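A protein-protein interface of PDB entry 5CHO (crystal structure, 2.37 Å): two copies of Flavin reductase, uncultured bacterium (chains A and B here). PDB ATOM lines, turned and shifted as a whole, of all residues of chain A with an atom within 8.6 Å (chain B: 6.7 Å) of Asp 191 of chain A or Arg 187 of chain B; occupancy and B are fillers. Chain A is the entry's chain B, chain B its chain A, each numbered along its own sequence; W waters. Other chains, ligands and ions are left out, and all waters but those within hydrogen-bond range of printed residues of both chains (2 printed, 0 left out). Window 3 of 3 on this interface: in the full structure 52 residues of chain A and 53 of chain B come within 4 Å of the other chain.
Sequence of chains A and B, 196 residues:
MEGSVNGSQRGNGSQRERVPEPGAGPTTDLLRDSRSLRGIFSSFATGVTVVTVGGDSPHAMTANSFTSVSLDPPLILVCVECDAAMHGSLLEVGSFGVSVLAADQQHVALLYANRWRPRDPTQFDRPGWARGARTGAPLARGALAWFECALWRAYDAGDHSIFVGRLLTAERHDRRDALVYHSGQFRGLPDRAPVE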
ATOM      1  N   ALA A  45       8.318   9.441 -25.254  1.00  0.00           N
ATOM      2  CA  ALA A  45       7.392   8.847 -24.296  1.00  0.00           C
ATOM      3  C   ALA A  45       6.149   8.263 -24.978  1.00  0.00           C
ATOM      4  O   ALA A  45       5.724   8.728 -26.038  1.00  0.00           O
ATOM      5  CB  ALA A  45       6.976   9.881 -23.263  1.00  0.00           C
ATOM      6  N   ALA A 103      -1.963   3.436 -14.761  1.00  0.00           N
ATOM      7  CA  ALA A 103      -0.662   3.307 -14.113  1.00  0.00           C
ATOM      8  C   ALA A 103      -0.594   2.120 -13.140  1.00  0.00           C
ATOM      9  O   ALA A 103       0.484   1.580 -12.889  1.00  0.00           O
ATOM     10  CB  ALA A 103      -0.309   4.599 -13.390  1.00  0.00           C
ATOM     11  N   LEU A 144      -7.887   2.557 -19.125  1.00  0.00           N
ATOM     12  CA  LEU A 144      -8.295   3.919 -19.440  1.00  0.00           C
ATOM     13  C   LEU A 144      -9.247   3.948 -20.631  1.00  0.00           C
ATOM     14  O   LEU A 144     -10.103   4.824 -20.730  1.00  0.00           O
ATOM     15  CB  LEU A 144      -7.061   4.768 -19.728  1.00  0.00           C
ATOM     16  CG  LEU A 144      -6.083   4.924 -18.563  1.00  0.00           C
ATOM     17  CD1 LEU A 144      -4.910   5.774 -18.994  1.00  0.00           C
ATOM     18  CD2 LEU A 144      -6.777   5.548 -17.357  1.00  0.00           C
ATOM     19  N   ARG A 172     -14.165   5.142 -23.698  1.00  0.00           N
ATOM     20  CA  ARG A 172     -13.286   5.729 -22.708  1.00  0.00           C
ATOM     21  C   ARG A 172     -13.873   5.545 -21.321  1.00  0.00           C
ATOM     22  O   ARG A 172     -15.069   5.745 -21.103  1.00  0.00           O
ATOM     23  CB  ARG A 172     -13.061   7.210 -22.987  1.00  0.00           C
ATOM     24  CG  ARG A 172     -11.968   7.778 -22.130  1.00  0.00           C
ATOM     25  CD  ARG A 172     -11.586   9.174 -22.527  1.00  0.00           C
ATOM     26  NE  ARG A 172     -10.355   9.542 -21.844  1.00  0.00           N
ATOM     27  CZ  ARG A 172      -9.797  10.744 -21.881  1.00  0.00           C
ATOM     28  NH1 ARG A 172     -10.368  11.732 -22.561  1.00  0.00           N
ATOM     29  NH2 ARG A 172      -8.666  10.955 -21.222  1.00  0.00           N
ATOM     30  N   HIS A 173     -13.012   5.160 -20.390  1.00  0.00           N
ATOM     31  CA  HIS A 173     -13.412   4.947 -19.011  1.00  0.00           C
ATOM     32  C   HIS A 173     -12.927   6.098 -18.156  1.00  0.00           C
ATOM     33  O   HIS A 173     -12.412   7.092 -18.670  1.00  0.00           O
ATOM     34  CB  HIS A 173     -12.860   3.623 -18.489  1.00  0.00           C
ATOM     35  CG  HIS A 173     -13.214   2.449 -19.348  1.00  0.00           C
ATOM     36  ND1 HIS A 173     -14.516   2.103 -19.629  1.00  0.00           N
ATOM     37  CD2 HIS A 173     -12.434   1.555 -20.000  1.00  0.00           C
ATOM     38  CE1 HIS A 173     -14.526   1.036 -20.410  1.00  0.00           C
ATOM     39  NE2 HIS A 173     -13.277   0.685 -20.649  1.00  0.00           N
ATOM     40  N   ASP A 174     -13.110   5.957 -16.851  1.00  0.00           N
ATOM     41  CA  ASP A 174     -12.715   6.982 -15.902  1.00  0.00           C
ATOM     42  C   ASP A 174     -11.273   7.400 -16.122  1.00  0.00           C
ATOM     43  O   ASP A 174     -10.391   6.558 -16.293  1.00  0.00           O
ATOM     44  CB  ASP A 174     -12.887   6.477 -14.468  1.00  0.00           C
ATOM     45  CG  ASP A 174     -14.338   6.438 -14.031  1.00  0.00           C
ATOM     46  OD1 ASP A 174     -15.193   7.029 -14.724  1.00  0.00           O
ATOM     47  OD2 ASP A 174     -14.625   5.806 -12.992  1.00  0.00           O
ATOM     48  N   ARG A 175     -11.038   8.705 -16.130  1.00  0.00           N
ATOM     49  CA  ARG A 175      -9.682   9.204 -16.214  1.00  0.00           C
ATOM     50  C   ARG A 175      -9.024   9.004 -14.866  1.00  0.00           C
ATOM     51  O   ARG A 175      -9.554   9.415 -13.834  1.00  0.00           O
ATOM     52  CB  ARG A 175      -9.659  10.673 -16.616  1.00  0.00           C
ATOM     53  CG  ARG A 175     -10.110  10.897 -18.038  1.00  0.00           C
ATOM     54  CD  ARG A 175     -10.309  12.367 -18.321  1.00  0.00           C
ATOM     55  NE  ARG A 175      -9.110  13.151 -18.035  1.00  0.00           N
ATOM     56  CZ  ARG A 175      -9.056  14.477 -18.102  1.00  0.00           C
ATOM     57  NH1 ARG A 175     -10.132  15.171 -18.445  1.00  0.00           N
ATOM     58  NH2 ARG A 175      -7.923  15.109 -17.825  1.00  0.00           N
ATOM     59  N   ARG A 176      -7.863   8.368 -14.890  1.00  0.00           N
ATOM     60  CA  ARG A 176      -7.032   8.224 -13.709  1.00  0.00           C
ATOM     61  C   ARG A 176      -5.607   8.127 -14.210  1.00  0.00           C
ATOM     62  O   ARG A 176      -5.380   8.185 -15.418  1.00  0.00           O
ATOM     63  CB  ARG A 176      -7.420   6.993 -12.883  1.00  0.00           C
ATOM     64  CG  ARG A 176      -7.568   5.694 -13.670  1.00  0.00           C
ATOM     65  CD  ARG A 176      -8.596   4.774 -13.022  1.00  0.00           C
ATOM     66  NE  ARG A 176      -8.349   3.374 -13.364  1.00  0.00           N
ATOM     67  CZ  ARG A 176      -7.372   2.643 -12.834  1.00  0.00           C
ATOM     68  NH1 ARG A 176      -6.544   3.179 -11.944  1.00  0.00           N
ATOM     69  NH2 ARG A 176      -7.215   1.378 -13.201  1.00  0.00           N
ATOM     70  N   ASP A 177      -4.652   7.995 -13.296  1.00  0.00           N
ATOM     71  CA  ASP A 177      -3.245   7.982 -13.671  1.00  0.00           C
ATOM     72  C   ASP A 177      -2.966   6.967 -14.775  1.00  0.00           C
ATOM     73  O   ASP A 177      -3.461   5.840 -14.743  1.00  0.00           O
ATOM     74  CB  ASP A 177      -2.371   7.694 -12.454  1.00  0.00           C
ATOM     75  CG  ASP A 177      -2.393   8.825 -11.448  1.00  0.00           C
ATOM     76  OD1 ASP A 177      -3.312   9.670 -11.526  1.00  0.00           O
ATOM     77  OD2 ASP A 177      -1.492   8.877 -10.584  1.00  0.00           O
ATOM     78  N   ALA A 178      -2.174   7.391 -15.756  1.00  0.00           N
ATOM     79  CA  ALA A 178      -1.911   6.594 -16.943  1.00  0.00           C
ATOM     80  C   ALA A 178      -0.533   5.957 -16.866  1.00  0.00           C
ATOM     81  O   ALA A 178       0.389   6.523 -16.281  1.00  0.00           O
ATOM     82  CB  ALA A 178      -2.031   7.458 -18.198  1.00  0.00           C
ATOM     83  N   LEU A 179      -0.399   4.777 -17.461  1.00  0.00           N
ATOM     84  CA  LEU A 179       0.888   4.098 -17.511  1.00  0.00           C
ATOM     85  C   LEU A 179       1.687   4.656 -18.674  1.00  0.00           C
ATOM     86  O   LEU A 179       1.201   4.707 -19.805  1.00  0.00           O
ATOM     87  CB  LEU A 179       0.717   2.585 -17.661  1.00  0.00           C
ATOM     88  CG  LEU A 179       2.004   1.767 -17.517  1.00  0.00           C
ATOM     89  CD1 LEU A 179       2.621   1.955 -16.134  1.00  0.00           C
ATOM     90  CD2 LEU A 179       1.753   0.292 -17.794  1.00  0.00           C
ATOM     91  N   GLY A 188       4.292   6.649 -13.986  1.00  0.00           N
ATOM     92  CA  GLY A 188       2.899   7.004 -13.788  1.00  0.00           C
ATOM     93  C   GLY A 188       2.694   8.458 -14.168  1.00  0.00           C
ATOM     94  O   GLY A 188       3.449   9.323 -13.728  1.00  0.00           O
ATOM     95  N   LEU A 189       1.680   8.724 -14.985  1.00  0.00           N
ATOM     96  CA  LEU A 189       1.332  10.088 -15.373  1.00  0.00           C
ATOM     97  C   LEU A 189       0.053  10.522 -14.673  1.00  0.00           C
ATOM     98  O   LEU A 189      -1.012   9.966 -14.933  1.00  0.00           O
ATOM     99  CB  LEU A 189       1.167  10.206 -16.889  1.00  0.00           C
ATOM    100  CG  LEU A 189       0.756  11.600 -17.387  1.00  0.00           C
ATOM    101  CD1 LEU A 189       1.904  12.586 -17.298  1.00  0.00           C
ATOM    102  CD2 LEU A 189       0.255  11.519 -18.820  1.00  0.00           C
ATOM    103  N   PRO A 190       0.151  11.514 -13.772  1.00  0.00           N
ATOM    104  CA  PRO A 190      -1.068  11.891 -13.056  1.00  0.00           C
ATOM    105  C   PRO A 190      -2.136  12.461 -13.977  1.00  0.00           C
ATOM    106  O   PRO A 190      -1.833  13.210 -14.907  1.00  0.00           O
ATOM    107  CB  PRO A 190      -0.587  12.967 -12.074  1.00  0.00           C
ATOM    108  CG  PRO A 190       0.880  12.796 -11.979  1.00  0.00           C
ATOM    109  CD  PRO A 190       1.311  12.306 -13.323  1.00  0.00           C
ATOM    110  N   ASP A 191      -3.382  12.097 -13.711  1.00  0.00           N
ATOM    111  CA  ASP A 191      -4.515  12.632 -14.448  1.00  0.00           C
ATOM    112  C   ASP A 191      -5.759  12.438 -13.606  1.00  0.00           C
ATOM    113  O   ASP A 191      -5.876  11.460 -12.871  1.00  0.00           O
ATOM    114  CB  ASP A 191      -4.675  11.953 -15.814  1.00  0.00           C
ATOM    115  CG  ASP A 191      -5.695  12.658 -16.704  1.00  0.00           C
ATOM    116  OD1 ASP A 191      -5.782  13.901 -16.640  1.00  0.00           O
ATOM    117  OD2 ASP A 191      -6.410  11.971 -17.467  1.00  0.00           O
ATOM    118  N   ARG A 192      -6.683  13.383 -13.721  1.00  0.00           N
ATOM    119  CA  ARG A 192      -7.947  13.338 -13.008  1.00  0.00           C
ATOM    120  C   ARG A 192      -8.949  14.063 -13.880  1.00  0.00           C
ATOM    121  O   ARG A 192      -8.583  14.997 -14.593  1.00  0.00           O
ATOM    122  CB  ARG A 192      -7.839  13.986 -11.624  1.00  0.00           C
ATOM    123  N   ALA A 193     -10.202  13.626 -13.844  1.00  0.00           N
ATOM    124  CA  ALA A 193     -11.254  14.301 -14.595  1.00  0.00           C
ATOM    125  C   ALA A 193     -11.303  15.790 -14.271  1.00  0.00           C
ATOM    126  O   ALA A 193     -11.568  16.180 -13.136  1.00  0.00           O
ATOM    127  CB  ALA A 193     -12.598  13.662 -14.313  1.00  0.00           C
ATOM    128  N   ALA B 103      10.174  19.281 -22.203  1.00  0.00           N
ATOM    129  CA  ALA B 103       9.008  19.862 -21.548  1.00  0.00           C
ATOM    130  C   ALA B 103       8.974  21.393 -21.632  1.00  0.00           C
ATOM    131  O   ALA B 103       7.897  21.992 -21.627  1.00  0.00           O
ATOM    132  CB  ALA B 103       8.968  19.415 -20.091  1.00  0.00           C
ATOM    133  N   GLN B 106       7.171  23.366 -25.022  1.00  0.00           N
ATOM    134  CA  GLN B 106       5.740  23.395 -25.273  1.00  0.00           C
ATOM    135  C   GLN B 106       5.377  24.468 -26.292  1.00  0.00           C
ATOM    136  O   GLN B 106       4.504  24.266 -27.137  1.00  0.00           O
ATOM    137  CB  GLN B 106       4.993  23.639 -23.967  1.00  0.00           C
ATOM    138  CG  GLN B 106       3.493  23.760 -24.112  1.00  0.00           C
ATOM    139  CD  GLN B 106       2.784  23.786 -22.771  1.00  0.00           C
ATOM    140  OE1 GLN B 106       3.131  23.044 -21.851  1.00  0.00           O
ATOM    141  NE2 GLN B 106       1.793  24.654 -22.651  1.00  0.00           N
ATOM    142  N   ALA B 178      10.375  15.771 -20.148  1.00  0.00           N
ATOM    143  CA  ALA B 178       9.845  15.528 -21.480  1.00  0.00           C
ATOM    144  C   ALA B 178       8.468  16.142 -21.667  1.00  0.00           C
ATOM    145  O   ALA B 178       7.672  16.215 -20.730  1.00  0.00           O
ATOM    146  CB  ALA B 178       9.787  14.034 -21.740  1.00  0.00           C
ATOM    147  N   LEU B 179       8.191  16.569 -22.893  1.00  0.00           N
ATOM    148  CA  LEU B 179       6.880  17.094 -23.235  1.00  0.00           C
ATOM    149  C   LEU B 179       5.975  15.933 -23.578  1.00  0.00           C
ATOM    150  O   LEU B 179       6.302  15.105 -24.429  1.00  0.00           O
ATOM    151  CB  LEU B 179       6.959  18.080 -24.398  1.00  0.00           C
ATOM    152  CG  LEU B 179       5.655  18.817 -24.713  1.00  0.00           C
ATOM    153  CD1 LEU B 179       5.191  19.624 -23.512  1.00  0.00           C
ATOM    154  CD2 LEU B 179       5.825  19.722 -25.928  1.00  0.00           C
ATOM    155  N   VAL B 180       4.833  15.883 -22.908  1.00  0.00           N
ATOM    156  CA  VAL B 180       3.880  14.809 -23.100  1.00  0.00           C
ATOM    157  C   VAL B 180       2.510  15.386 -23.411  1.00  0.00           C
ATOM    158  O   VAL B 180       2.109  16.401 -22.841  1.00  0.00           O
ATOM    159  CB  VAL B 180       3.840  13.906 -21.852  1.00  0.00           C
ATOM    160  CG1 VAL B 180       2.619  12.998 -21.856  1.00  0.00           C
ATOM    161  CG2 VAL B 180       5.124  13.093 -21.781  1.00  0.00           C
ATOM    162  N   TYR B 181       1.800  14.728 -24.321  1.00  0.00           N
ATOM    163  CA  TYR B 181       0.463  15.145 -24.709  1.00  0.00           C
ATOM    164  C   TYR B 181      -0.533  14.064 -24.329  1.00  0.00           C
ATOM    165  O   TYR B 181      -0.520  12.970 -24.893  1.00  0.00           O
ATOM    166  CB  TYR B 181       0.403  15.431 -26.211  1.00  0.00           C
ATOM    167  CG  TYR B 181      -0.900  16.037 -26.663  1.00  0.00           C
ATOM    168  CD1 TYR B 181      -1.278  17.304 -26.244  1.00  0.00           C
ATOM    169  CD2 TYR B 181      -1.747  15.348 -27.521  1.00  0.00           C
ATOM    170  CE1 TYR B 181      -2.474  17.867 -26.661  1.00  0.00           C
ATOM    171  CE2 TYR B 181      -2.939  15.901 -27.945  1.00  0.00           C
ATOM    172  CZ  TYR B 181      -3.297  17.160 -27.511  1.00  0.00           C
ATOM    173  OH  TYR B 181      -4.484  17.714 -27.923  1.00  0.00           O
ATOM    174  N   HIS B 182      -1.392  14.378 -23.364  1.00  0.00           N
ATOM    175  CA  HIS B 182      -2.362  13.416 -22.853  1.00  0.00           C
ATOM    176  C   HIS B 182      -3.664  14.083 -22.422  1.00  0.00           C
ATOM    177  O   HIS B 182      -3.651  15.157 -21.818  1.00  0.00           O
ATOM    178  CB  HIS B 182      -1.773  12.649 -21.673  1.00  0.00           C
ATOM    179  CG  HIS B 182      -2.709  11.638 -21.094  1.00  0.00           C
ATOM    180  ND1 HIS B 182      -3.314  11.801 -19.867  1.00  0.00           N
ATOM    181  CD2 HIS B 182      -3.142  10.447 -21.572  1.00  0.00           C
ATOM    182  CE1 HIS B 182      -4.085  10.758 -19.618  1.00  0.00           C
ATOM    183  NE2 HIS B 182      -3.996   9.921 -20.637  1.00  0.00           N
ATOM    184  N   SER B 183      -4.784  13.438 -22.742  1.00  0.00           N
ATOM    185  CA  SER B 183      -6.111  13.964 -22.432  1.00  0.00           C
ATOM    186  C   SER B 183      -6.271  15.365 -23.002  1.00  0.00           C
ATOM    187  O   SER B 183      -6.943  16.212 -22.416  1.00  0.00           O
ATOM    188  CB  SER B 183      -6.360  13.964 -20.916  1.00  0.00           C
ATOM    189  OG  SER B 183      -6.889  12.725 -20.491  1.00  0.00           O
ATOM    190  N   GLN B 185      -4.135  17.580 -23.100  1.00  0.00           N
ATOM    191  CA  GLN B 185      -3.329  18.514 -22.319  1.00  0.00           C
ATOM    192  C   GLN B 185      -1.856  18.297 -22.570  1.00  0.00           C
ATOM    193  O   GLN B 185      -1.420  17.170 -22.804  1.00  0.00           O
ATOM    194  CB  GLN B 185      -3.588  18.363 -20.817  1.00  0.00           C
ATOM    195  CG  GLN B 185      -4.987  18.689 -20.337  1.00  0.00           C
ATOM    196  CD  GLN B 185      -5.351  20.138 -20.568  1.00  0.00           C
ATOM    197  OE1 GLN B 185      -4.540  21.033 -20.328  1.00  0.00           O
ATOM    198  NE2 GLN B 185      -6.589  20.381 -20.985  1.00  0.00           N
ATOM    199  N   PHE B 186      -1.088  19.381 -22.514  1.00  0.00           N
ATOM    200  CA  PHE B 186       0.357  19.260 -22.513  1.00  0.00           C
ATOM    201  C   PHE B 186       0.804  19.060 -21.069  1.00  0.00           C
ATOM    202  O   PHE B 186       0.291  19.707 -20.152  1.00  0.00           O
ATOM    203  CB  PHE B 186       1.023  20.484 -23.149  1.00  0.00           C
ATOM    204  CG  PHE B 186       0.862  20.541 -24.640  1.00  0.00           C
ATOM    205  CD1 PHE B 186      -0.136  21.308 -25.217  1.00  0.00           C
ATOM    206  CD2 PHE B 186       1.696  19.805 -25.462  1.00  0.00           C
ATOM    207  CE1 PHE B 186      -0.290  21.348 -26.587  1.00  0.00           C
ATOM    208  CE2 PHE B 186       1.549  19.841 -26.833  1.00  0.00           C
ATOM    209  CZ  PHE B 186       0.554  20.615 -27.398  1.00  0.00           C
ATOM    210  N   ARG B 187       1.763  18.159 -20.882  1.00  0.00           N
ATOM    211  CA  ARG B 187       2.251  17.811 -19.555  1.00  0.00           C
ATOM    212  C   ARG B 187       3.755  17.709 -19.576  1.00  0.00           C
ATOM    213  O   ARG B 187       4.367  17.502 -20.627  1.00  0.00           O
ATOM    214  CB  ARG B 187       1.658  16.486 -19.057  1.00  0.00           C
ATOM    215  CG  ARG B 187       0.154  16.487 -19.014  1.00  0.00           C
ATOM    216  CD  ARG B 187      -0.356  17.344 -17.860  1.00  0.00           C
ATOM    217  NE  ARG B 187      -1.811  17.450 -17.875  1.00  0.00           N
ATOM    218  CZ  ARG B 187      -2.658  16.637 -17.256  1.00  0.00           C
ATOM    219  NH1 ARG B 187      -2.231  15.686 -16.438  1.00  0.00           N
ATOM    220  NH2 ARG B 187      -3.958  16.831 -17.414  1.00  0.00           N
ATOM    221  N   GLY B 188       4.341  17.887 -18.401  1.00  0.00           N
ATOM    222  CA  GLY B 188       5.762  17.688 -18.223  1.00  0.00           C
ATOM    223  C   GLY B 188       5.977  16.356 -17.539  1.00  0.00           C
ATOM    224  O   GLY B 188       5.378  16.077 -16.502  1.00  0.00           O
ATOM    225  N   LEU B 189       6.845  15.539 -18.123  1.00  0.00           N
ATOM    226  CA  LEU B 189       7.201  14.249 -17.548  1.00  0.00           C
ATOM    227  C   LEU B 189       8.609  14.361 -16.983  1.00  0.00           C
ATOM    228  O   LEU B 189       9.558  14.541 -17.744  1.00  0.00           O
ATOM    229  CB  LEU B 189       7.132  13.139 -18.595  1.00  0.00           C
ATOM    230  CG  LEU B 189       7.478  11.746 -18.059  1.00  0.00           C
ATOM    231  CD1 LEU B 189       6.314  11.158 -17.259  1.00  0.00           C
ATOM    232  CD2 LEU B 189       7.907  10.815 -19.179  1.00  0.00           C
HETATM  233  O   HOH W   1       0.004  15.165 -15.228  1.00  0.00           O
HETATM  234  O   HOH W   2      -2.568  13.448 -18.043  1.00  0.00           O
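OG of Ser 183 of chain B lies within hydrogen-bond range of OD2 of Asp 191 of chain A (3.2 Å).
OG of Ser 183 of chain B sits at hydrogen-bond distance from NH2 of Arg 172 of chain A, at 2.6 Å.
NH2 of Arg 187 of chain B is in salt-bridge range of OD1 of Asp 191 of chain A, at 3.5 Å.
NH1 of Arg 187 of chain B sits at hydrogen-bond distance from O of Pro 190 of chain A (2.9 Å).
The side-chain hydroxyl of Ser 183 of chain B is in hydrogen-bond range of the guanidinium group of Arg 175 of chain A (3.3 Å).
OD1 of Asp 191 of chain A is in salt-bridge range of NH2 of Arg 175 of chain A (2.7 Å).
N of Leu 189 of chain A is in hydrogen-bond range of O of Ala 178 of chain A (2.9 Å).
The guanidinium group (NH2) of Arg 175 of chain A sits at hydrogen-bond distance from the backbone carbonyl oxygen (O) of Arg 192 of chain A (3.3 Å).
OD1 of Asp 177 of chain A lies within hydrogen-bond range of N of Asp 191 of chain A (3.3 Å).
The backbone carbonyl oxygen of Val 180 of chain B lies within hydrogen-bond range of the backbone NH of Arg 187 of chain B, at 2.7 Å.
Among the printed residues, pairs that only touch across the chains: Ala 45 of chain A with Val 180 of chain B (3.99 Å), Ala 178 of chain A with His 182 of chain B (3.98 Å), Leu 189 of chain A with His 182 of chain B (3.7 Å) and Asp 191 of chain A with His 182 of chain B (3.4 Å).
Printed residues of chain B within 4 Å of Arg 172 of chain A: Ser 183.
Of the printed residues of chain B, Arg 175 of chain A touches Ser 183 (3.3 Å).
Of chain A, only Pro 190 (2.9 Å) and Asp 191 (3.5 Å) come within 4 Å of Arg 187 of chain B.
No residue of chain A comes within 4 Å of Gly 188 of chain B.
The nearest residue of chain A that does not touch Arg 187 of chain B is Leu 189 of chain A (4.3 Å).
The nearest printed residue of chain A that does not touch Ser 183 of chain B is Arg 192 of chain A (6.5 Å).
Printed residues of chain A that touch a printed residue of chain B: Ala 45, Arg 172, Arg 175, Ala 178, Leu 189, Pro 190 and Asp 191.
Among the printed residues, 9 pairs touch across the chains.
Positions printed for both chains: 103, 178, 179, 188 and 189.
Of the 9 pairs that touch across the chains among the printed residues, none has its exchanged pair printed and touching as well.
Water W2 lies within hydrogen-bond range of a ring nitrogen (ND1) of His 182 of chain B (2.6 Å), the guanidinium group of Arg 187 of chain B (2.8 Å) and the backbone carbonyl oxygen of Pro 190 of chain A (3.2 Å).
Water W1 bridges the guanidinium group of Arg 187 of chain B and the backbone carbonyl oxygen of Pro 190 of chain A.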
